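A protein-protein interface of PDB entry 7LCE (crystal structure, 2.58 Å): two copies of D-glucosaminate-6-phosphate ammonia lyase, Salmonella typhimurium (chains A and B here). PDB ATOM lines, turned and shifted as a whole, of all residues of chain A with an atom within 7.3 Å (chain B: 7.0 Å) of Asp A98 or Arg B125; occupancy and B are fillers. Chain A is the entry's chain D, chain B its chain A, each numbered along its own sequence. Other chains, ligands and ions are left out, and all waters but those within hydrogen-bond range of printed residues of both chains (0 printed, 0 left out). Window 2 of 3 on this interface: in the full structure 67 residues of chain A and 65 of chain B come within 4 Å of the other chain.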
ATOM      1  N   ILE A  85      23.254  -6.797  38.235  1.00  0.00           N
ATOM      2  CA  ILE A  85      23.309  -6.229  36.892  1.00  0.00           C
ATOM      3  C   ILE A  85      21.908  -6.031  36.327  1.00  0.00           C
ATOM      4  O   ILE A  85      21.610  -4.991  35.729  1.00  0.00           O
ATOM      5  CB  ILE A  85      24.166  -7.127  35.981  1.00  0.00           C
ATOM      6  CG1 ILE A  85      25.613  -7.166  36.475  1.00  0.00           C
ATOM      7  CG2 ILE A  85      24.097  -6.662  34.533  1.00  0.00           C
ATOM      8  CD1 ILE A  85      26.517  -8.015  35.626  1.00  0.00           C
ATOM      9  N   ARG A  92      16.396  -8.066  31.046  1.00  0.00           N
ATOM     10  CA  ARG A  92      17.814  -8.233  31.345  1.00  0.00           C
ATOM     11  C   ARG A  92      18.125  -9.628  31.879  1.00  0.00           C
ATOM     12  O   ARG A  92      19.221 -10.148  31.640  1.00  0.00           O
ATOM     13  CB  ARG A  92      18.276  -7.180  32.353  1.00  0.00           C
ATOM     14  CG  ARG A  92      18.421  -5.754  31.840  1.00  0.00           C
ATOM     15  CD  ARG A  92      18.833  -4.854  33.005  1.00  0.00           C
ATOM     16  NE  ARG A  92      19.830  -3.848  32.652  1.00  0.00           N
ATOM     17  CZ  ARG A  92      19.567  -2.682  32.082  1.00  0.00           C
ATOM     18  NH1 ARG A  92      18.333  -2.333  31.756  1.00  0.00           N
ATOM     19  NH2 ARG A  92      20.567  -1.839  31.840  1.00  0.00           N
ATOM     20  N   VAL A  93      17.185 -10.246  32.597  1.00  0.00           N
ATOM     21  CA  VAL A  93      17.414 -11.593  33.113  1.00  0.00           C
ATOM     22  C   VAL A  93      17.575 -12.580  31.966  1.00  0.00           C
ATOM     23  O   VAL A  93      18.441 -13.465  32.001  1.00  0.00           O
ATOM     24  CB  VAL A  93      16.277 -12.005  34.068  1.00  0.00           C
ATOM     25  CG1 VAL A  93      16.257 -13.510  34.258  1.00  0.00           C
ATOM     26  CG2 VAL A  93      16.452 -11.317  35.411  1.00  0.00           C
ATOM     27  N   ALA A  94      16.753 -12.438  30.924  1.00  0.00           N
ATOM     28  CA  ALA A  94      16.856 -13.314  29.764  1.00  0.00           C
ATOM     29  C   ALA A  94      18.128 -13.067  28.963  1.00  0.00           C
ATOM     30  O   ALA A  94      18.553 -13.947  28.210  1.00  0.00           O
ATOM     31  CB  ALA A  94      15.634 -13.144  28.863  1.00  0.00           C
ATOM     32  N   LEU A  95      18.739 -11.889  29.103  1.00  0.00           N
ATOM     33  CA  LEU A  95      19.942 -11.572  28.347  1.00  0.00           C
ATOM     34  C   LEU A  95      21.208 -12.154  28.960  1.00  0.00           C
ATOM     35  O   LEU A  95      22.203 -12.319  28.245  1.00  0.00           O
ATOM     36  CB  LEU A  95      20.095 -10.058  28.212  1.00  0.00           C
ATOM     37  CG  LEU A  95      19.365  -9.457  27.014  1.00  0.00           C
ATOM     38  CD1 LEU A  95      19.699  -7.982  26.866  1.00  0.00           C
ATOM     39  CD2 LEU A  95      19.716 -10.225  25.752  1.00  0.00           C
ATOM     40  N   MET A  96      21.204 -12.451  30.256  1.00  0.00           N
ATOM     41  CA  MET A  96      22.421 -12.917  30.902  1.00  0.00           C
ATOM     42  C   MET A  96      22.880 -14.229  30.270  1.00  0.00           C
ATOM     43  O   MET A  96      22.048 -15.072  29.914  1.00  0.00           O
ATOM     44  CB  MET A  96      22.195 -13.102  32.401  1.00  0.00           C
ATOM     45  CG  MET A  96      21.811 -11.827  33.131  1.00  0.00           C
ATOM     46  SD  MET A  96      23.120 -10.585  33.119  1.00  0.00           S
ATOM     47  CE  MET A  96      22.590  -9.506  31.783  1.00  0.00           C
ATOM     48  N   PRO A  97      24.197 -14.435  30.110  1.00  0.00           N
ATOM     49  CA  PRO A  97      25.236 -13.520  30.592  1.00  0.00           C
ATOM     50  C   PRO A  97      25.714 -12.468  29.586  1.00  0.00           C
ATOM     51  O   PRO A  97      26.853 -12.018  29.713  1.00  0.00           O
ATOM     52  CB  PRO A  97      26.387 -14.468  30.944  1.00  0.00           C
ATOM     53  CG  PRO A  97      26.120 -15.742  30.151  1.00  0.00           C
ATOM     54  CD  PRO A  97      24.784 -15.618  29.466  1.00  0.00           C
ATOM     55  N   ASP A  98      24.882 -12.082  28.617  1.00  0.00           N
ATOM     56  CA  ASP A  98      25.250 -11.033  27.661  1.00  0.00           C
ATOM     57  C   ASP A  98      24.826  -9.681  28.222  1.00  0.00           C
ATOM     58  O   ASP A  98      23.739  -9.176  27.940  1.00  0.00           O
ATOM     59  CB  ASP A  98      24.624 -11.292  26.296  1.00  0.00           C
ATOM     60  CG  ASP A  98      24.969 -10.213  25.276  1.00  0.00           C
ATOM     61  OD1 ASP A  98      25.828  -9.355  25.569  1.00  0.00           O
ATOM     62  OD2 ASP A  98      24.377 -10.223  24.177  1.00  0.00           O
ATOM     63  N   SER A  99      25.704  -9.091  29.030  1.00  0.00           N
ATOM     64  CA  SER A  99      25.510  -7.784  29.659  1.00  0.00           C
ATOM     65  C   SER A  99      26.158  -6.663  28.852  1.00  0.00           C
ATOM     66  O   SER A  99      26.782  -5.769  29.427  1.00  0.00           O
ATOM     67  CB  SER A  99      26.054  -7.805  31.081  1.00  0.00           C
ATOM     68  OG  SER A  99      27.450  -8.046  31.073  1.00  0.00           O
ATOM     69  N   SER A 100      26.009  -6.678  27.525  1.00  0.00           N
ATOM     70  CA  SER A 100      26.768  -5.774  26.661  1.00  0.00           C
ATOM     71  C   SER A 100      26.512  -4.303  26.982  1.00  0.00           C
ATOM     72  O   SER A 100      27.419  -3.582  27.413  1.00  0.00           O
ATOM     73  CB  SER A 100      26.430  -6.063  25.197  1.00  0.00           C
ATOM     74  OG  SER A 100      26.882  -7.348  24.812  1.00  0.00           O
ATOM     75  N   GLY A 101      25.289  -3.835  26.768  1.00  0.00           N
ATOM     76  CA  GLY A 101      24.986  -2.435  26.991  1.00  0.00           C
ATOM     77  C   GLY A 101      24.693  -2.014  28.411  1.00  0.00           C
ATOM     78  O   GLY A 101      24.230  -0.890  28.623  1.00  0.00           O
ATOM     79  N   MET A 102      24.975  -2.854  29.397  1.00  0.00           N
ATOM     80  CA  MET A 102      24.621  -2.571  30.778  1.00  0.00           C
ATOM     81  C   MET A 102      25.847  -2.239  31.617  1.00  0.00           C
ATOM     82  O   MET A 102      26.993  -2.453  31.215  1.00  0.00           O
ATOM     83  CB  MET A 102      23.909  -3.784  31.382  1.00  0.00           C
ATOM     84  CG  MET A 102      22.898  -4.416  30.457  1.00  0.00           C
ATOM     85  SD  MET A 102      22.228  -5.925  31.161  1.00  0.00           S
ATOM     86  CE  MET A 102      21.246  -6.522  29.786  1.00  0.00           C
ATOM     87  N   ASN A 104      28.063  -3.483  34.140  1.00  0.00           N
ATOM     88  CA  ASN A 104      28.358  -4.869  34.479  1.00  0.00           C
ATOM     89  C   ASN A 104      29.686  -5.068  35.198  1.00  0.00           C
ATOM     90  O   ASN A 104      30.077  -6.217  35.430  1.00  0.00           O
ATOM     91  CB  ASN A 104      28.334  -5.728  33.212  1.00  0.00           C
ATOM     92  CG  ASN A 104      29.213  -5.167  32.112  1.00  0.00           C
ATOM     93  OD1 ASN A 104      30.088  -4.333  32.357  1.00  0.00           O
ATOM     94  ND2 ASN A 104      28.984  -5.625  30.892  1.00  0.00           N
ATOM     95  N   ARG A 125      31.539 -14.205  35.864  1.00  0.00           N
ATOM     96  CA  ARG A 125      31.265 -14.044  34.440  1.00  0.00           C
ATOM     97  C   ARG A 125      29.972 -14.737  34.038  1.00  0.00           C
ATOM     98  O   ARG A 125      29.310 -14.305  33.087  1.00  0.00           O
ATOM     99  CB  ARG A 125      32.431 -14.577  33.609  1.00  0.00           C
ATOM    100  CG  ARG A 125      32.578 -13.897  32.255  1.00  0.00           C
ATOM    101  CD  ARG A 125      33.644 -14.573  31.397  1.00  0.00           C
ATOM    102  NE  ARG A 125      34.988 -14.386  31.931  1.00  0.00           N
ATOM    103  CZ  ARG A 125      35.688 -15.337  32.537  1.00  0.00           C
ATOM    104  NH1 ARG A 125      35.208 -16.562  32.684  1.00  0.00           N
ATOM    105  NH2 ARG A 125      36.900 -15.051  33.006  1.00  0.00           N
ATOM    106  N   LEU A 126      29.603 -15.817  34.734  1.00  0.00           N
ATOM    107  CA  LEU A 126      28.339 -16.479  34.437  1.00  0.00           C
ATOM    108  C   LEU A 126      27.158 -15.576  34.750  1.00  0.00           C
ATOM    109  O   LEU A 126      26.111 -15.676  34.101  1.00  0.00           O
ATOM    110  CB  LEU A 126      28.225 -17.783  35.223  1.00  0.00           C
ATOM    111  CG  LEU A 126      28.965 -18.988  34.652  1.00  0.00           C
ATOM    112  CD1 LEU A 126      28.854 -20.165  35.605  1.00  0.00           C
ATOM    113  CD2 LEU A 126      28.416 -19.344  33.283  1.00  0.00           C
ATOM    114  N   GLY A 127      27.302 -14.698  35.738  1.00  0.00           N
ATOM    115  CA  GLY A 127      26.281 -13.724  36.052  1.00  0.00           C
ATOM    116  C   GLY A 127      26.294 -12.500  35.169  1.00  0.00           C
ATOM    117  O   GLY A 127      25.455 -11.610  35.338  1.00  0.00           O
ATOM    118  N   GLY A 128      27.234 -12.427  34.229  1.00  0.00           N
ATOM    119  CA  GLY A 128      27.339 -11.305  33.324  1.00  0.00           C
ATOM    120  C   GLY A 128      28.331 -10.245  33.738  1.00  0.00           C
ATOM    121  O   GLY A 128      28.427  -9.213  33.062  1.00  0.00           O
ATOM    122  N   ILE A 240      19.636 -17.647  34.131  1.00  0.00           N
ATOM    123  CA  ILE A 240      20.811 -18.489  34.311  1.00  0.00           C
ATOM    124  C   ILE A 240      20.643 -19.464  35.466  1.00  0.00           C
ATOM    125  O   ILE A 240      21.341 -20.484  35.512  1.00  0.00           O
ATOM    126  CB  ILE A 240      22.070 -17.628  34.520  1.00  0.00           C
ATOM    127  CG1 ILE A 240      21.977 -16.853  35.831  1.00  0.00           C
ATOM    128  CG2 ILE A 240      22.259 -16.673  33.354  1.00  0.00           C
ATOM    129  CD1 ILE A 240      23.277 -16.185  36.232  1.00  0.00           C
ATOM    130  N   ILE B  77      22.847 -28.943  28.653  1.00  0.00           N
ATOM    131  CA  ILE B  77      22.904 -28.168  27.419  1.00  0.00           C
ATOM    132  C   ILE B  77      24.039 -27.155  27.482  1.00  0.00           C
ATOM    133  O   ILE B  77      24.820 -27.014  26.533  1.00  0.00           O
ATOM    134  CB  ILE B  77      21.549 -27.488  27.147  1.00  0.00           C
ATOM    135  CG1 ILE B  77      20.464 -28.543  26.916  1.00  0.00           C
ATOM    136  CG2 ILE B  77      21.653 -26.537  25.964  1.00  0.00           C
ATOM    137  CD1 ILE B  77      19.087 -27.963  26.693  1.00  0.00           C
ATOM    138  N   ALA B  78      24.151 -26.438  28.602  1.00  0.00           N
ATOM    139  CA  ALA B  78      25.213 -25.446  28.739  1.00  0.00           C
ATOM    140  C   ALA B  78      26.590 -26.092  28.681  1.00  0.00           C
ATOM    141  O   ALA B  78      27.493 -25.583  28.006  1.00  0.00           O
ATOM    142  CB  ALA B  78      25.043 -24.673  30.045  1.00  0.00           C
ATOM    143  N   VAL B  81      27.461 -27.465  25.070  1.00  0.00           N
ATOM    144  CA  VAL B  81      27.857 -26.383  24.172  1.00  0.00           C
ATOM    145  C   VAL B  81      29.271 -25.921  24.497  1.00  0.00           C
ATOM    146  O   VAL B  81      30.108 -25.746  23.602  1.00  0.00           O
ATOM    147  CB  VAL B  81      26.849 -25.223  24.247  1.00  0.00           C
ATOM    148  CG1 VAL B  81      27.366 -24.020  23.476  1.00  0.00           C
ATOM    149  CG2 VAL B  81      25.507 -25.663  23.694  1.00  0.00           C
ATOM    150  N   PRO B  97      31.686 -17.911  30.017  1.00  0.00           N
ATOM    151  CA  PRO B  97      31.049 -17.961  28.700  1.00  0.00           C
ATOM    152  C   PRO B  97      31.473 -16.857  27.733  1.00  0.00           C
ATOM    153  O   PRO B  97      30.704 -16.542  26.824  1.00  0.00           O
ATOM    154  CB  PRO B  97      29.561 -17.821  29.038  1.00  0.00           C
ATOM    155  CG  PRO B  97      29.519 -17.168  30.422  1.00  0.00           C
ATOM    156  CD  PRO B  97      30.931 -17.059  30.944  1.00  0.00           C
ATOM    157  N   ASP B  98      32.668 -16.293  27.903  1.00  0.00           N
ATOM    158  CA  ASP B  98      33.175 -15.279  26.976  1.00  0.00           C
ATOM    159  C   ASP B  98      33.901 -16.018  25.860  1.00  0.00           C
ATOM    160  O   ASP B  98      35.118 -16.210  25.898  1.00  0.00           O
ATOM    161  CB  ASP B  98      34.085 -14.283  27.686  1.00  0.00           C
ATOM    162  CG  ASP B  98      34.640 -13.213  26.748  1.00  0.00           C
ATOM    163  OD1 ASP B  98      34.193 -13.137  25.585  1.00  0.00           O
ATOM    164  OD2 ASP B  98      35.526 -12.442  27.178  1.00  0.00           O
ATOM    165  N   SER B  99      33.142 -16.418  24.843  1.00  0.00           N
ATOM    166  CA  SER B  99      33.684 -17.165  23.710  1.00  0.00           C
ATOM    167  C   SER B  99      34.112 -16.256  22.573  1.00  0.00           C
ATOM    168  O   SER B  99      33.935 -16.596  21.400  1.00  0.00           O
ATOM    169  CB  SER B  99      32.650 -18.173  23.224  1.00  0.00           C
ATOM    170  OG  SER B  99      31.497 -17.500  22.749  1.00  0.00           O
ATOM    171  N   PRO B 119      14.069 -20.084  28.480  1.00  0.00           N
ATOM    172  CA  PRO B 119      14.430 -20.326  27.080  1.00  0.00           C
ATOM    173  C   PRO B 119      15.663 -21.209  26.964  1.00  0.00           C
ATOM    174  O   PRO B 119      16.631 -21.062  27.715  1.00  0.00           O
ATOM    175  CB  PRO B 119      14.700 -18.919  26.533  1.00  0.00           C
ATOM    176  CG  PRO B 119      13.991 -17.998  27.479  1.00  0.00           C
ATOM    177  CD  PRO B 119      14.131 -18.653  28.820  1.00  0.00           C
ATOM    178  N   VAL B 120      15.615 -22.143  26.008  1.00  0.00           N
ATOM    179  CA  VAL B 120      16.770 -22.984  25.720  1.00  0.00           C
ATOM    180  C   VAL B 120      17.958 -22.142  25.278  1.00  0.00           C
ATOM    181  O   VAL B 120      19.107 -22.591  25.364  1.00  0.00           O
ATOM    182  CB  VAL B 120      16.402 -24.044  24.659  1.00  0.00           C
ATOM    183  CG1 VAL B 120      16.044 -23.374  23.339  1.00  0.00           C
ATOM    184  CG2 VAL B 120      17.521 -25.062  24.482  1.00  0.00           C
ATOM    185  N   THR B 121      17.707 -20.915  24.813  1.00  0.00           N
ATOM    186  CA  THR B 121      18.794 -20.014  24.446  1.00  0.00           C
ATOM    187  C   THR B 121      19.648 -19.648  25.651  1.00  0.00           C
ATOM    188  O   THR B 121      20.863 -19.460  25.516  1.00  0.00           O
ATOM    189  CB  THR B 121      18.235 -18.743  23.806  1.00  0.00           C
ATOM    190  OG1 THR B 121      17.711 -17.885  24.829  1.00  0.00           O
ATOM    191  CG2 THR B 121      17.119 -19.083  22.836  1.00  0.00           C
ATOM    192  N   SER B 122      19.036 -19.534  26.834  1.00  0.00           N
ATOM    193  CA  SER B 122      19.793 -19.164  28.025  1.00  0.00           C
ATOM    194  C   SER B 122      20.839 -20.218  28.361  1.00  0.00           C
ATOM    195  O   SER B 122      21.987 -19.887  28.675  1.00  0.00           O
ATOM    196  CB  SER B 122      18.850 -18.949  29.207  1.00  0.00           C
ATOM    197  OG  SER B 122      18.113 -17.749  29.051  1.00  0.00           O
ATOM    198  N   ALA B 123      20.464 -21.497  28.296  1.00  0.00           N
ATOM    199  CA  ALA B 123      21.440 -22.550  28.550  1.00  0.00           C
ATOM    200  C   ALA B 123      22.542 -22.524  27.498  1.00  0.00           C
ATOM    201  O   ALA B 123      23.725 -22.681  27.822  1.00  0.00           O
ATOM    202  CB  ALA B 123      20.749 -23.913  28.586  1.00  0.00           C
ATOM    203  N   ILE B 124      22.170 -22.311  26.233  1.00  0.00           N
ATOM    204  CA  ILE B 124      23.162 -22.228  25.166  1.00  0.00           C
ATOM    205  C   ILE B 124      24.096 -21.045  25.391  1.00  0.00           C
ATOM    206  O   ILE B 124      25.314 -21.153  25.200  1.00  0.00           O
ATOM    207  CB  ILE B 124      22.459 -22.151  23.797  1.00  0.00           C
ATOM    208  CG1 ILE B 124      21.665 -23.431  23.542  1.00  0.00           C
ATOM    209  CG2 ILE B 124      23.463 -21.926  22.684  1.00  0.00           C
ATOM    210  CD1 ILE B 124      20.647 -23.302  22.437  1.00  0.00           C
ATOM    211  N   ARG B 125      23.548 -19.897  25.804  1.00  0.00           N
ATOM    212  CA  ARG B 125      24.393 -18.725  26.014  1.00  0.00           C
ATOM    213  C   ARG B 125      25.335 -18.907  27.197  1.00  0.00           C
ATOM    214  O   ARG B 125      26.432 -18.336  27.206  1.00  0.00           O
ATOM    215  CB  ARG B 125      23.537 -17.472  26.214  1.00  0.00           C
ATOM    216  CG  ARG B 125      24.240 -16.179  25.800  1.00  0.00           C
ATOM    217  CD  ARG B 125      23.433 -14.931  26.167  1.00  0.00           C
ATOM    218  NE  ARG B 125      22.215 -14.787  25.378  1.00  0.00           N
ATOM    219  CZ  ARG B 125      20.994 -15.012  25.843  1.00  0.00           C
ATOM    220  NH1 ARG B 125      20.789 -15.382  27.097  1.00  0.00           N
ATOM    221  NH2 ARG B 125      19.952 -14.858  25.030  1.00  0.00           N
ATOM    222  N   LEU B 126      24.931 -19.686  28.205  1.00  0.00           N
ATOM    223  CA  LEU B 126      25.818 -19.941  29.336  1.00  0.00           C
ATOM    224  C   LEU B 126      27.045 -20.737  28.918  1.00  0.00           C
ATOM    225  O   LEU B 126      28.118 -20.576  29.507  1.00  0.00           O
ATOM    226  CB  LEU B 126      25.072 -20.685  30.442  1.00  0.00           C
ATOM    227  CG  LEU B 126      24.178 -19.875  31.375  1.00  0.00           C
ATOM    228  CD1 LEU B 126      23.432 -20.812  32.303  1.00  0.00           C
ATOM    229  CD2 LEU B 126      24.995 -18.873  32.165  1.00  0.00           C
ATOM    230  N   GLY B 127      26.909 -21.597  27.915  1.00  0.00           N
ATOM    231  CA  GLY B 127      28.040 -22.341  27.404  1.00  0.00           C
ATOM    232  C   GLY B 127      28.912 -21.586  26.434  1.00  0.00           C
ATOM    233  O   GLY B 127      29.908 -22.134  25.951  1.00  0.00           O
ATOM    234  N   GLY B 128      28.560 -20.339  26.125  1.00  0.00           N
ATOM    235  CA  GLY B 128      29.316 -19.525  25.199  1.00  0.00           C
ATOM    236  C   GLY B 128      28.793 -19.533  23.782  1.00  0.00           C
ATOM    237  O   GLY B 128      29.415 -18.919  22.908  1.00  0.00           O
ATOM    238  N   GLY B 129      27.670 -20.202  23.529  1.00  0.00           N
ATOM    239  CA  GLY B 129      27.185 -20.343  22.174  1.00  0.00           C
ATOM    240  C   GLY B 129      26.381 -19.140  21.718  1.00  0.00           C
ATOM    241  O   GLY B 129      25.740 -18.450  22.507  1.00  0.00           O
ATOM    242  N   ARG B 130      26.461 -18.867  20.419  1.00  0.00           N
ATOM    243  CA  ARG B 130      25.614 -17.889  19.754  1.00  0.00           C
ATOM    244  C   ARG B 130      24.686 -18.632  18.803  1.00  0.00           C
ATOM    245  O   ARG B 130      25.149 -19.417  17.968  1.00  0.00           O
ATOM    246  CB  ARG B 130      26.460 -16.855  19.007  1.00  0.00           C
ATOM    247  CG  ARG B 130      27.381 -16.069  19.930  1.00  0.00           C
ATOM    248  CD  ARG B 130      28.242 -15.074  19.177  1.00  0.00           C
ATOM    249  NE  ARG B 130      27.437 -14.109  18.441  1.00  0.00           N
ATOM    250  CZ  ARG B 130      27.004 -12.966  18.954  1.00  0.00           C
ATOM    251  NH1 ARG B 130      27.280 -12.622  20.203  1.00  0.00           N
ATOM    252  NH2 ARG B 130      26.278 -12.147  18.198  1.00  0.00           N
ATOM    253  N   ILE B 131      23.384 -18.398  18.936  1.00  0.00           N
ATOM    254  CA  ILE B 131      22.388 -19.195  18.226  1.00  0.00           C
ATOM    255  C   ILE B 131      22.291 -18.744  16.774  1.00  0.00           C
ATOM    256  O   ILE B 131      22.230 -17.544  16.484  1.00  0.00           O
ATOM    257  CB  ILE B 131      21.023 -19.105  18.924  1.00  0.00           C
ATOM    258  CG1 ILE B 131      21.084 -19.815  20.276  1.00  0.00           C
ATOM    259  CG2 ILE B 131      19.929 -19.703  18.046  1.00  0.00           C
ATOM    260  CD1 ILE B 131      19.739 -20.255  20.786  1.00  0.00           C
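Of the printed residues of chain B, Ala A94 touches Ser B122 and Arg B125.
Of the printed residues of chain B, Pro A97 touches Pro B97, Arg B125 and Leu B126.
Asp A98 touches just one residue of chain B: Arg B125 (3.8 Å).
Of the printed residues of chain B, Leu A126 touches Pro B97 and Leu B126.
Ile B77 touches none of the printed residues of chain A.
Printed residues of chain A within 4 Å of Asp B98: Arg A125.
Of the printed residues of chain A, Ser B122 touches Ala A94.
Of chain A, only Ala A94, Leu A95, Met A96, Pro A97 and Asp A98 come within 4 Å of Arg B125.
The nearest residue of chain B that does not touch Asp A98 is Arg B130 (5.5 Å).
The nearest printed residue of chain A that does not touch Leu B126 is Met A96 (5.3 Å).
The guanidinium group (NH1) of Arg B125 lies within hydrogen-bond range of the backbone carbonyl oxygen (O) of Met A96 (3.1 Å).
NH1 of Arg B125 is in hydrogen-bond range of O of Ala A94.
Pro B97 touches its own counterpart, Pro A97.
Pro A97 touches Arg B125, and with the chains exchanged Arg A125 touches Pro B97.
Pro A97 touches Leu B126, and with the chains exchanged Leu A126 touches Pro B97.
Asp A98 touches Arg B125, and with the chains exchanged Arg A125 touches Asp B98.
7 positions are printed for both chains.
Of the 13 pairs that touch across the chains among the printed residues, 8 have their exchanged pair printed and touching as well.
Of the 19 printed residues of chain B, 5 touch a printed residue of chain A.
Printed residues of chain B that touch a printed residue of chain A: Pro B97, Asp B98, Ser B122, Arg B125 and Leu B126.
The side-chain carboxylate of Asp A98 lies close to the backbone NH of Ser A100.
Among the printed residues, merely in contact across the chains: Leu A95 with Arg B125, Leu A126 with Leu B126, Pro A97 with Arg B125, Pro A97 with Pro B97, Ile A240 with Leu B126, Arg A125 with Pro B97, Arg A125 with Asp B98, Leu A126 with Pro B97, Asp A98 with Arg B125, Pro A97 with Leu B126 and Ala A94 with Ser B122.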
